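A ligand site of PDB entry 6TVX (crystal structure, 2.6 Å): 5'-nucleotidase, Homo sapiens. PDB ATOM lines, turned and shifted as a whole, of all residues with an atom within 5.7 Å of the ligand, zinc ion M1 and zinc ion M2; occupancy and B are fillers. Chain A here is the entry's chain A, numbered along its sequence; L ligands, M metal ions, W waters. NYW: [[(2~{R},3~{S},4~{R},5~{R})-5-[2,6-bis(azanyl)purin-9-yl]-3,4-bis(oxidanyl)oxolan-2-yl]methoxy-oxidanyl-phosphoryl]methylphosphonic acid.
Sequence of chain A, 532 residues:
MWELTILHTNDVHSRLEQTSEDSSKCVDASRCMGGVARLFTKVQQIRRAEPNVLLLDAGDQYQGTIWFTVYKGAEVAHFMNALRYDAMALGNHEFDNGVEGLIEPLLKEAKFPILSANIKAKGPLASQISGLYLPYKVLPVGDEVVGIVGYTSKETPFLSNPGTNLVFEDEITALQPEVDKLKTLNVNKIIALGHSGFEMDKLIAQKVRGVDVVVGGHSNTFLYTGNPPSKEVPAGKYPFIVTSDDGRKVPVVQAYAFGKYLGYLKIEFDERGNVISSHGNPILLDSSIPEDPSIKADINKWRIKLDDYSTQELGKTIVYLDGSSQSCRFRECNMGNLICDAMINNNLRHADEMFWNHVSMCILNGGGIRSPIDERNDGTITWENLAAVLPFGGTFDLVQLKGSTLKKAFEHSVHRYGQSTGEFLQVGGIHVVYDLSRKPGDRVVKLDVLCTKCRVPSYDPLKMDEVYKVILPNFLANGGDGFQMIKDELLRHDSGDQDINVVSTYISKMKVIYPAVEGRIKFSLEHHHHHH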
ATOM      1  N   ASP A  11     -18.875 -17.288   5.646  1.00  0.00           N
ATOM      2  CA  ASP A  11     -18.998 -17.694   4.251  1.00  0.00           C
ATOM      3  C   ASP A  11     -18.591 -19.148   4.058  1.00  0.00           C
ATOM      4  O   ASP A  11     -17.773 -19.450   3.209  1.00  0.00           O
ATOM      5  CB  ASP A  11     -18.193 -16.718   3.411  1.00  0.00           C
ATOM      6  CG  ASP A  11     -18.442 -15.299   3.887  1.00  0.00           C
ATOM      7  OD1 ASP A  11     -19.598 -14.959   4.100  1.00  0.00           O
ATOM      8  OD2 ASP A  11     -17.461 -14.574   4.137  1.00  0.00           O
ATOM      9  N   HIS A  13     -20.673 -21.508   3.108  1.00  0.00           N
ATOM     10  CA  HIS A  13     -21.343 -21.810   1.835  1.00  0.00           C
ATOM     11  C   HIS A  13     -21.441 -23.310   1.493  1.00  0.00           C
ATOM     12  O   HIS A  13     -20.868 -23.778   0.509  1.00  0.00           O
ATOM     13  CB  HIS A  13     -20.676 -21.025   0.691  1.00  0.00           C
ATOM     14  CG  HIS A  13     -20.953 -19.566   0.747  1.00  0.00           C
ATOM     15  ND1 HIS A  13     -22.244 -19.058   0.679  1.00  0.00           N
ATOM     16  CD2 HIS A  13     -20.095 -18.522   0.827  1.00  0.00           C
ATOM     17  CE1 HIS A  13     -22.134 -17.748   0.750  1.00  0.00           C
ATOM     18  NE2 HIS A  13     -20.853 -17.377   0.823  1.00  0.00           N
ATOM     19  N   ASP A  60     -23.597 -16.584   6.276  1.00  0.00           N
ATOM     20  CA  ASP A  60     -23.485 -17.226   4.963  1.00  0.00           C
ATOM     21  C   ASP A  60     -23.098 -18.720   5.049  1.00  0.00           C
ATOM     22  O   ASP A  60     -22.121 -19.157   4.441  1.00  0.00           O
ATOM     23  CB  ASP A  60     -22.557 -16.439   4.023  1.00  0.00           C
ATOM     24  CG  ASP A  60     -23.185 -15.350   3.170  1.00  0.00           C
ATOM     25  OD1 ASP A  60     -24.331 -14.944   3.475  1.00  0.00           O
ATOM     26  OD2 ASP A  60     -22.512 -14.873   2.244  1.00  0.00           O
ATOM     27  N   GLY A  91     -26.640 -14.000   7.715  1.00  0.00           N
ATOM     28  CA  GLY A  91     -26.013 -13.422   6.539  1.00  0.00           C
ATOM     29  C   GLY A  91     -27.052 -13.330   5.453  1.00  0.00           C
ATOM     30  O   GLY A  91     -28.114 -13.940   5.571  1.00  0.00           O
ATOM     31  N   ASN A  92     -26.793 -12.557   4.402  1.00  0.00           N
ATOM     32  CA  ASN A  92     -27.755 -12.360   3.318  1.00  0.00           C
ATOM     33  C   ASN A  92     -28.207 -13.655   2.621  1.00  0.00           C
ATOM     34  O   ASN A  92     -29.354 -13.732   2.193  1.00  0.00           O
ATOM     35  CB  ASN A  92     -27.221 -11.368   2.273  1.00  0.00           C
ATOM     36  CG  ASN A  92     -25.915 -11.798   1.621  1.00  0.00           C
ATOM     37  OD1 ASN A  92     -24.953 -12.186   2.304  1.00  0.00           O
ATOM     38  ND2 ASN A  92     -25.842 -11.753   0.302  1.00  0.00           N
ATOM     39  N   HIS A  93     -27.324 -14.666   2.529  1.00  0.00           N
ATOM     40  CA  HIS A  93     -27.675 -15.924   1.864  1.00  0.00           C
ATOM     41  C   HIS A  93     -28.624 -16.792   2.683  1.00  0.00           C
ATOM     42  O   HIS A  93     -29.221 -17.709   2.127  1.00  0.00           O
ATOM     43  CB  HIS A  93     -26.428 -16.700   1.409  1.00  0.00           C
ATOM     44  CG  HIS A  93     -25.791 -16.092   0.203  1.00  0.00           C
ATOM     45  ND1 HIS A  93     -25.896 -14.741  -0.069  1.00  0.00           N
ATOM     46  CD2 HIS A  93     -25.037 -16.668  -0.769  1.00  0.00           C
ATOM     47  CE1 HIS A  93     -25.255 -14.546  -1.208  1.00  0.00           C
ATOM     48  NE2 HIS A  93     -24.672 -15.665  -1.626  1.00  0.00           N
ATOM     49  N   LEU A 159     -29.490  -7.776  -2.319  1.00  0.00           N
ATOM     50  CA  LEU A 159     -28.644  -8.957  -2.564  1.00  0.00           C
ATOM     51  C   LEU A 159     -29.374 -10.296  -2.505  1.00  0.00           C
ATOM     52  O   LEU A 159     -28.921 -11.241  -3.144  1.00  0.00           O
ATOM     53  CB  LEU A 159     -27.461  -8.991  -1.585  1.00  0.00           C
ATOM     54  CG  LEU A 159     -26.501  -7.810  -1.612  1.00  0.00           C
ATOM     55  CD1 LEU A 159     -25.545  -7.879  -0.447  1.00  0.00           C
ATOM     56  CD2 LEU A 159     -25.728  -7.760  -2.929  1.00  0.00           C
ATOM     57  N   HIS A 195     -22.486  -9.918   9.600  1.00  0.00           N
ATOM     58  CA  HIS A 195     -22.239 -10.211   8.192  1.00  0.00           C
ATOM     59  C   HIS A 195     -22.395  -8.972   7.277  1.00  0.00           C
ATOM     60  O   HIS A 195     -23.393  -8.868   6.572  1.00  0.00           O
ATOM     61  CB  HIS A 195     -23.193 -11.339   7.768  1.00  0.00           C
ATOM     62  CG  HIS A 195     -22.927 -11.857   6.399  1.00  0.00           C
ATOM     63  ND1 HIS A 195     -21.953 -12.797   6.168  1.00  0.00           N
ATOM     64  CD2 HIS A 195     -23.495 -11.515   5.232  1.00  0.00           C
ATOM     65  CE1 HIS A 195     -21.964 -13.000   4.866  1.00  0.00           C
ATOM     66  NE2 HIS A 195     -22.894 -12.265   4.256  1.00  0.00           N
ATOM     67  N   HIS A 218     -18.839 -11.832   5.064  1.00  0.00           N
ATOM     68  CA  HIS A 218     -19.324 -11.177   3.811  1.00  0.00           C
ATOM     69  C   HIS A 218     -18.238 -10.766   2.791  1.00  0.00           C
ATOM     70  O   HIS A 218     -18.508 -10.830   1.596  1.00  0.00           O
ATOM     71  CB  HIS A 218     -20.217  -9.975   4.095  1.00  0.00           C
ATOM     72  CG  HIS A 218     -20.985  -9.534   2.895  1.00  0.00           C
ATOM     73  ND1 HIS A 218     -22.091 -10.213   2.453  1.00  0.00           N
ATOM     74  CD2 HIS A 218     -20.738  -8.506   2.046  1.00  0.00           C
ATOM     75  CE1 HIS A 218     -22.512  -9.570   1.381  1.00  0.00           C
ATOM     76  NE2 HIS A 218     -21.733  -8.537   1.100  1.00  0.00           N
ATOM     77  N   SER A 219     -17.058 -10.291   3.223  1.00  0.00           N
ATOM     78  CA  SER A 219     -15.998  -9.863   2.303  1.00  0.00           C
ATOM     79  C   SER A 219     -14.961 -10.972   1.972  1.00  0.00           C
ATOM     80  O   SER A 219     -14.025 -10.692   1.219  1.00  0.00           O
ATOM     81  CB  SER A 219     -15.307  -8.618   2.853  1.00  0.00           C
ATOM     82  OG  SER A 219     -15.065  -8.724   4.256  1.00  0.00           O
ATOM     83  N   ASN A 220     -15.141 -12.216   2.500  1.00  0.00           N
ATOM     84  CA  ASN A 220     -14.196 -13.347   2.338  1.00  0.00           C
ATOM     85  C   ASN A 220     -12.760 -12.897   2.664  1.00  0.00           C
ATOM     86  O   ASN A 220     -11.801 -13.308   1.986  1.00  0.00           O
ATOM     87  CB  ASN A 220     -14.274 -13.960   0.942  1.00  0.00           C
ATOM     88  CG  ASN A 220     -15.656 -14.373   0.507  1.00  0.00           C
ATOM     89  OD1 ASN A 220     -16.460 -14.826   1.321  1.00  0.00           O
ATOM     90  ND2 ASN A 220     -15.952 -14.254  -0.787  1.00  0.00           N
ATOM     91  N   ARG A 329     -12.856 -12.064 -10.834  1.00  0.00           N
ATOM     92  CA  ARG A 329     -13.188 -10.707 -10.420  1.00  0.00           C
ATOM     93  C   ARG A 329     -12.103  -9.699 -10.786  1.00  0.00           C
ATOM     94  O   ARG A 329     -12.307  -8.508 -10.551  1.00  0.00           O
ATOM     95  CB  ARG A 329     -13.492 -10.659  -8.924  1.00  0.00           C
ATOM     96  CG  ARG A 329     -14.507 -11.707  -8.538  1.00  0.00           C
ATOM     97  CD  ARG A 329     -15.100 -11.481  -7.185  1.00  0.00           C
ATOM     98  NE  ARG A 329     -16.046 -12.553  -6.868  1.00  0.00           N
ATOM     99  CZ  ARG A 329     -16.897 -12.528  -5.841  1.00  0.00           C
ATOM    100  NH1 ARG A 329     -16.947 -11.474  -5.034  1.00  0.00           N
ATOM    101  NH2 ARG A 329     -17.711 -13.559  -5.631  1.00  0.00           N
ATOM    102  N   ASN A 365     -21.407 -11.291 -14.746  1.00  0.00           N
ATOM    103  CA  ASN A 365     -20.716 -10.793 -13.551  1.00  0.00           C
ATOM    104  C   ASN A 365     -19.847 -11.895 -12.895  1.00  0.00           C
ATOM    105  O   ASN A 365     -20.323 -12.990 -12.640  1.00  0.00           O
ATOM    106  CB  ASN A 365     -21.736 -10.206 -12.564  1.00  0.00           C
ATOM    107  CG  ASN A 365     -22.795 -11.161 -12.077  1.00  0.00           C
ATOM    108  OD1 ASN A 365     -23.707 -11.531 -12.814  1.00  0.00           O
ATOM    109  ND2 ASN A 365     -22.682 -11.629 -10.858  1.00  0.00           N
ATOM    110  N   GLY A 366     -18.569 -11.576 -12.642  1.00  0.00           N
ATOM    111  CA  GLY A 366     -17.604 -12.499 -12.033  1.00  0.00           C
ATOM    112  C   GLY A 366     -17.992 -13.071 -10.683  1.00  0.00           C
ATOM    113  O   GLY A 366     -17.554 -14.173 -10.324  1.00  0.00           O
ATOM    114  N   GLY A 367     -18.815 -12.340  -9.931  1.00  0.00           N
ATOM    115  CA  GLY A 367     -19.329 -12.780  -8.642  1.00  0.00           C
ATOM    116  C   GLY A 367     -20.370 -13.887  -8.726  1.00  0.00           C
ATOM    117  O   GLY A 367     -20.605 -14.577  -7.745  1.00  0.00           O
ATOM    118  N   GLY A 368     -20.992 -14.040  -9.898  1.00  0.00           N
ATOM    119  CA  GLY A 368     -21.961 -15.085 -10.150  1.00  0.00           C
ATOM    120  C   GLY A 368     -21.306 -16.422 -10.409  1.00  0.00           C
ATOM    121  O   GLY A 368     -21.974 -17.460 -10.317  1.00  0.00           O
ATOM    122  N   ARG A 370     -19.027 -18.919  -8.880  1.00  0.00           N
ATOM    123  CA  ARG A 370     -18.700 -19.112  -7.466  1.00  0.00           C
ATOM    124  C   ARG A 370     -17.889 -20.365  -7.111  1.00  0.00           C
ATOM    125  O   ARG A 370     -17.672 -20.610  -5.919  1.00  0.00           O
ATOM    126  CB  ARG A 370     -20.003 -19.047  -6.686  1.00  0.00           C
ATOM    127  CG  ARG A 370     -20.429 -17.602  -6.593  1.00  0.00           C
ATOM    128  CD  ARG A 370     -21.710 -17.390  -5.862  1.00  0.00           C
ATOM    129  NE  ARG A 370     -21.591 -16.239  -4.952  1.00  0.00           N
ATOM    130  CZ  ARG A 370     -21.219 -16.289  -3.666  1.00  0.00           C
ATOM    131  NH1 ARG A 370     -21.148 -15.174  -2.957  1.00  0.00           N
ATOM    132  NH2 ARG A 370     -20.904 -17.453  -3.099  1.00  0.00           N
ATOM    133  N   PHE A 392     -27.164 -20.352  -7.660  1.00  0.00           N
ATOM    134  CA  PHE A 392     -28.357 -19.524  -7.463  1.00  0.00           C
ATOM    135  C   PHE A 392     -29.561 -19.887  -8.295  1.00  0.00           C
ATOM    136  O   PHE A 392     -30.651 -19.422  -7.979  1.00  0.00           O
ATOM    137  CB  PHE A 392     -28.017 -18.042  -7.667  1.00  0.00           C
ATOM    138  CG  PHE A 392     -26.878 -17.532  -6.815  1.00  0.00           C
ATOM    139  CD1 PHE A 392     -26.680 -18.001  -5.525  1.00  0.00           C
ATOM    140  CD2 PHE A 392     -26.021 -16.564  -7.295  1.00  0.00           C
ATOM    141  CE1 PHE A 392     -25.628 -17.525  -4.745  1.00  0.00           C
ATOM    142  CE2 PHE A 392     -24.977 -16.082  -6.515  1.00  0.00           C
ATOM    143  CZ  PHE A 392     -24.806 -16.556  -5.235  1.00  0.00           C
ATOM    144  N   SER A 420     -11.995  -7.063  -5.035  1.00  0.00           N
ATOM    145  CA  SER A 420     -12.578  -8.408  -5.163  1.00  0.00           C
ATOM    146  C   SER A 420     -14.115  -8.352  -5.268  1.00  0.00           C
ATOM    147  O   SER A 420     -14.802  -9.258  -4.805  1.00  0.00           O
ATOM    148  CB  SER A 420     -12.138  -9.327  -4.023  1.00  0.00           C
ATOM    149  OG  SER A 420     -12.249 -10.694  -4.364  1.00  0.00           O
ATOM    150  N   THR A 421     -14.644  -7.278  -5.899  1.00  0.00           N
ATOM    151  CA  THR A 421     -16.085  -7.093  -6.081  1.00  0.00           C
ATOM    152  C   THR A 421     -16.530  -7.847  -7.313  1.00  0.00           C
ATOM    153  O   THR A 421     -15.857  -7.828  -8.352  1.00  0.00           O
ATOM    154  CB  THR A 421     -16.434  -5.615  -6.136  1.00  0.00           C
ATOM    155  OG1 THR A 421     -15.699  -5.006  -7.200  1.00  0.00           O
ATOM    156  CG2 THR A 421     -16.184  -4.904  -4.817  1.00  0.00           C
ATOM    157  N   GLY A 422     -17.679  -8.492  -7.196  1.00  0.00           N
ATOM    158  CA  GLY A 422     -18.223  -9.327  -8.241  1.00  0.00           C
ATOM    159  C   GLY A 422     -18.819  -8.603  -9.435  1.00  0.00           C
ATOM    160  O   GLY A 422     -19.229  -9.290 -10.377  1.00  0.00           O
ATOM    161  N   GLU A 423     -18.850  -7.249  -9.427  1.00  0.00           N
ATOM    162  CA  GLU A 423     -19.379  -6.501 -10.580  1.00  0.00           C
ATOM    163  C   GLU A 423     -18.478  -6.597 -11.816  1.00  0.00           C
ATOM    164  O   GLU A 423     -18.944  -6.232 -12.892  1.00  0.00           O
ATOM    165  CB  GLU A 423     -19.721  -5.024 -10.215  1.00  0.00           C
ATOM    166  CG  GLU A 423     -18.602  -3.983 -10.330  1.00  0.00           C
ATOM    167  CD  GLU A 423     -17.861  -3.585  -9.065  1.00  0.00           C
ATOM    168  OE1 GLU A 423     -18.398  -3.806  -7.955  1.00  0.00           O
ATOM    169  OE2 GLU A 423     -16.757  -3.018  -9.204  1.00  0.00           O
ATOM    170  N   PRO A 473     -27.235 -12.648 -17.109  1.00  0.00           N
ATOM    171  CA  PRO A 473     -28.062 -13.128 -15.995  1.00  0.00           C
ATOM    172  C   PRO A 473     -29.184 -12.168 -15.627  1.00  0.00           C
ATOM    173  O   PRO A 473     -29.007 -10.954 -15.726  1.00  0.00           O
ATOM    174  CB  PRO A 473     -27.069 -13.249 -14.830  1.00  0.00           C
ATOM    175  CG  PRO A 473     -25.754 -13.277 -15.419  1.00  0.00           C
ATOM    176  CD  PRO A 473     -25.801 -12.621 -16.756  1.00  0.00           C
ATOM    177  N   ASN A 474     -30.334 -12.707 -15.169  1.00  0.00           N
ATOM    178  CA  ASN A 474     -31.479 -11.894 -14.721  1.00  0.00           C
ATOM    179  C   ASN A 474     -31.082 -10.953 -13.548  1.00  0.00           C
ATOM    180  O   ASN A 474     -31.741  -9.923 -13.352  1.00  0.00           O
ATOM    181  CB  ASN A 474     -32.668 -12.789 -14.307  1.00  0.00           C
ATOM    182  CG  ASN A 474     -32.458 -13.615 -13.039  1.00  0.00           C
ATOM    183  OD1 ASN A 474     -31.363 -14.131 -12.775  1.00  0.00           O
ATOM    184  ND2 ASN A 474     -33.510 -13.797 -12.247  1.00  0.00           N
ATOM    185  N   PHE A 475     -30.018 -11.319 -12.774  1.00  0.00           N
ATOM    186  CA  PHE A 475     -29.463 -10.519 -11.679  1.00  0.00           C
ATOM    187  C   PHE A 475     -29.008  -9.154 -12.193  1.00  0.00           C
ATOM    188  O   PHE A 475     -29.230  -8.132 -11.539  1.00  0.00           O
ATOM    189  CB  PHE A 475     -28.282 -11.267 -11.045  1.00  0.00           C
ATOM    190  CG  PHE A 475     -27.626 -10.530  -9.890  1.00  0.00           C
ATOM    191  CD1 PHE A 475     -28.306 -10.323  -8.699  1.00  0.00           C
ATOM    192  CD2 PHE A 475     -26.339 -10.036 -10.006  1.00  0.00           C
ATOM    193  CE1 PHE A 475     -27.714  -9.624  -7.644  1.00  0.00           C
ATOM    194  CE2 PHE A 475     -25.754  -9.331  -8.961  1.00  0.00           C
ATOM    195  CZ  PHE A 475     -26.447  -9.140  -7.781  1.00  0.00           C
ATOM    196  N   ASP A 481     -25.785  -5.648  -8.516  1.00  0.00           N
ATOM    197  CA  ASP A 481     -24.370  -5.264  -8.481  1.00  0.00           C
ATOM    198  C   ASP A 481     -24.142  -3.820  -8.947  1.00  0.00           C
ATOM    199  O   ASP A 481     -23.115  -3.498  -9.529  1.00  0.00           O
ATOM    200  CB  ASP A 481     -23.480  -6.293  -9.254  1.00  0.00           C
ATOM    201  CG  ASP A 481     -22.534  -7.120  -8.384  1.00  0.00           C
ATOM    202  OD1 ASP A 481     -22.406  -6.828  -7.160  1.00  0.00           O
ATOM    203  OD2 ASP A 481     -21.919  -8.062  -8.921  1.00  0.00           O
HETATM  204  C6  NYW L   1     -27.570 -13.534  -7.699  1.00  0.00           C
HETATM  205  C4  NYW L   1     -25.281 -12.942  -7.498  1.00  0.00           C
HETATM  206  C2  NYW L   1     -26.054 -13.714  -9.466  1.00  0.00           C
HETATM  207  PB  NYW L   1     -22.009 -12.990  -0.575  1.00  0.00           P
HETATM  208  O1B NYW L   1     -22.916 -12.451   0.484  1.00  0.00           O
HETATM  209  O2B NYW L   1     -22.685 -13.049  -1.957  1.00  0.00           O
HETATM  210  O3B NYW L   1     -21.563 -14.433  -0.238  1.00  0.00           O
HETATM  211  PA  NYW L   1     -19.382 -12.503  -2.090  1.00  0.00           P
HETATM  212  O1A NYW L   1     -18.583 -13.792  -1.986  1.00  0.00           O
HETATM  213  O2A NYW L   1     -18.347 -11.339  -2.166  1.00  0.00           O
HETATM  214  C3A NYW L   1     -20.514 -12.014  -0.795  1.00  0.00           C
HETATM  215  O5' NYW L   1     -20.302 -12.471  -3.365  1.00  0.00           O
HETATM  216  C5' NYW L   1     -20.856 -11.243  -3.885  1.00  0.00           C
HETATM  217  C4' NYW L   1     -21.296 -11.389  -5.314  1.00  0.00           C
HETATM  218  O4' NYW L   1     -22.315 -12.399  -5.457  1.00  0.00           O
HETATM  219  C3' NYW L   1     -21.943 -10.153  -5.895  1.00  0.00           C
HETATM  220  O3' NYW L   1     -20.971  -9.162  -6.233  1.00  0.00           O
HETATM  221  C2' NYW L   1     -22.749 -10.705  -7.082  1.00  0.00           C
HETATM  222  O2' NYW L   1     -22.047 -10.665  -8.321  1.00  0.00           O
HETATM  223  C1' NYW L   1     -23.009 -12.161  -6.676  1.00  0.00           C
HETATM  224  N9  NYW L   1     -24.422 -12.488  -6.521  1.00  0.00           N
HETATM  225  C8  NYW L   1     -25.193 -12.337  -5.392  1.00  0.00           C
HETATM  226  N7  NYW L   1     -26.458 -12.655  -5.565  1.00  0.00           N
HETATM  227  C5  NYW L   1     -26.520 -13.045  -6.889  1.00  0.00           C
HETATM  228  N6  NYW L   1     -28.830 -13.668  -7.270  1.00  0.00           N
HETATM  229  N1  NYW L   1     -27.327 -13.864  -8.988  1.00  0.00           N
HETATM  230  N3  NYW L   1     -24.976 -13.255  -8.766  1.00  0.00           N
HETATM  231  N2  NYW L   1     -25.829 -14.068 -10.735  1.00  0.00           N
HETATM  232 ZN    ZN M   1     -20.589 -15.531   1.400  1.00  0.00          ZN
HETATM  233 ZN    ZN M   2     -22.604 -12.406   2.340  1.00  0.00          ZN
HETATM  234  O   HOH W   1     -19.900 -13.821   1.743  1.00  0.00           O
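An oxygen (O1A) of the ligand lies within hydrogen-bond range of the side-chain amide nitrogen (ND2) of Asn 220, 2.9 Å away. The side-chain amide nitrogen (ND2) of Asn 365 lies within hydrogen-bond range of an oxygen (O2') of the ligand, 2.8 Å away. A ring nitrogen (NE2) of His 93 lies close to an oxygen (O2B) of the ligand, at 3.3 Å. O2B of the ligand lies within salt-bridge range of NH1 of Arg 370, at 2.8 Å. The side-chain carboxylate of Asp 481 lies within hydrogen-bond range of an oxygen (O2') of the ligand. N of Gly 422 lies close to O3' of the ligand, at 3.5 Å. O2A of the ligand lies within salt-bridge range of NH1 of Arg 329, at 3.2 Å.
OD2 of Asp 11 lies within hydrogen-bond range of N of His 218 (3.2 Å). The side-chain carboxylate of Asp 11 lies close to the side-chain amide oxygen of Asn 220, 3.0 Å away. The side-chain carboxylate (OD2) of Asp 481 sits at hydrogen-bond distance from the backbone NH (N) of Glu 423, 3.2 Å away. The guanidinium group (NE) of Arg 370 sits close to the backbone carbonyl oxygen (O) of Gly 367 (3.4 Å). The backbone NH (N) of His 93 lies within hydrogen-bond range of the side-chain carboxylate (OD1) of Asp 60. The backbone carbonyl oxygen (O) of Ser 420 lies within hydrogen-bond range of the guanidinium group (NH1) of Arg 329 (3.1 Å). The backbone NH of Gly 366 is in hydrogen-bond range of the backbone carbonyl oxygen of Gly 422. The backbone carbonyl oxygen (O) of Gly 422 lies within hydrogen-bond range of the backbone NH (N) of Gly 367, at 3.1 Å.
Residues that only touch the ligand: Leu 159 (3.7 Å), Gly 367 (3.5 Å), Gly 368 (3.8 Å), Phe 392 (3.3 Å) and Phe 475 (3.4 Å). Hydrophobic or aromatic side chains within 4 Å of the ligand: His 13, His 93, His 218, Phe 392 and Phe 475. Of the 26 residues printed, 17 come within 4 Å of the ligand. The nearest printed residue that does not touch the ligand is Glu 423 (4.3 Å).
Asp 11 touches zinc ion M1 (OD1 to ZN, 2.9 Å). The nearest printed residue that does not touch zinc ion M1 is Asn 220 (4.2 Å).
Four residues have an atom within 4 Å of zinc ion M2: Asp 60, Asn 92, His 195 and His 218.
Zinc ion M1 is bound by water W1 (1.9 Å), a ring nitrogen (NE2) of His 13 (2.0 Å), an oxygen (O3B) of the ligand (2.2 Å) and the side-chain carboxylate of Asp 60 (2.2 Å).
Zinc ion M2 is bound by an oxygen (O1B) of the ligand, a ring nitrogen (NE2) of His 195, a ring nitrogen (ND1) of His 218, the side-chain amide oxygen of Asn 92 and the side-chain carboxylate of Asp 60. Zinc ion M2 has five donor atoms within binding distance.
Water W1 bridges the side-chain carboxylate (OD1) of Asp 11 (2.6 Å) and the backbone carbonyl oxygen (O) of His 218 (3.3 Å).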
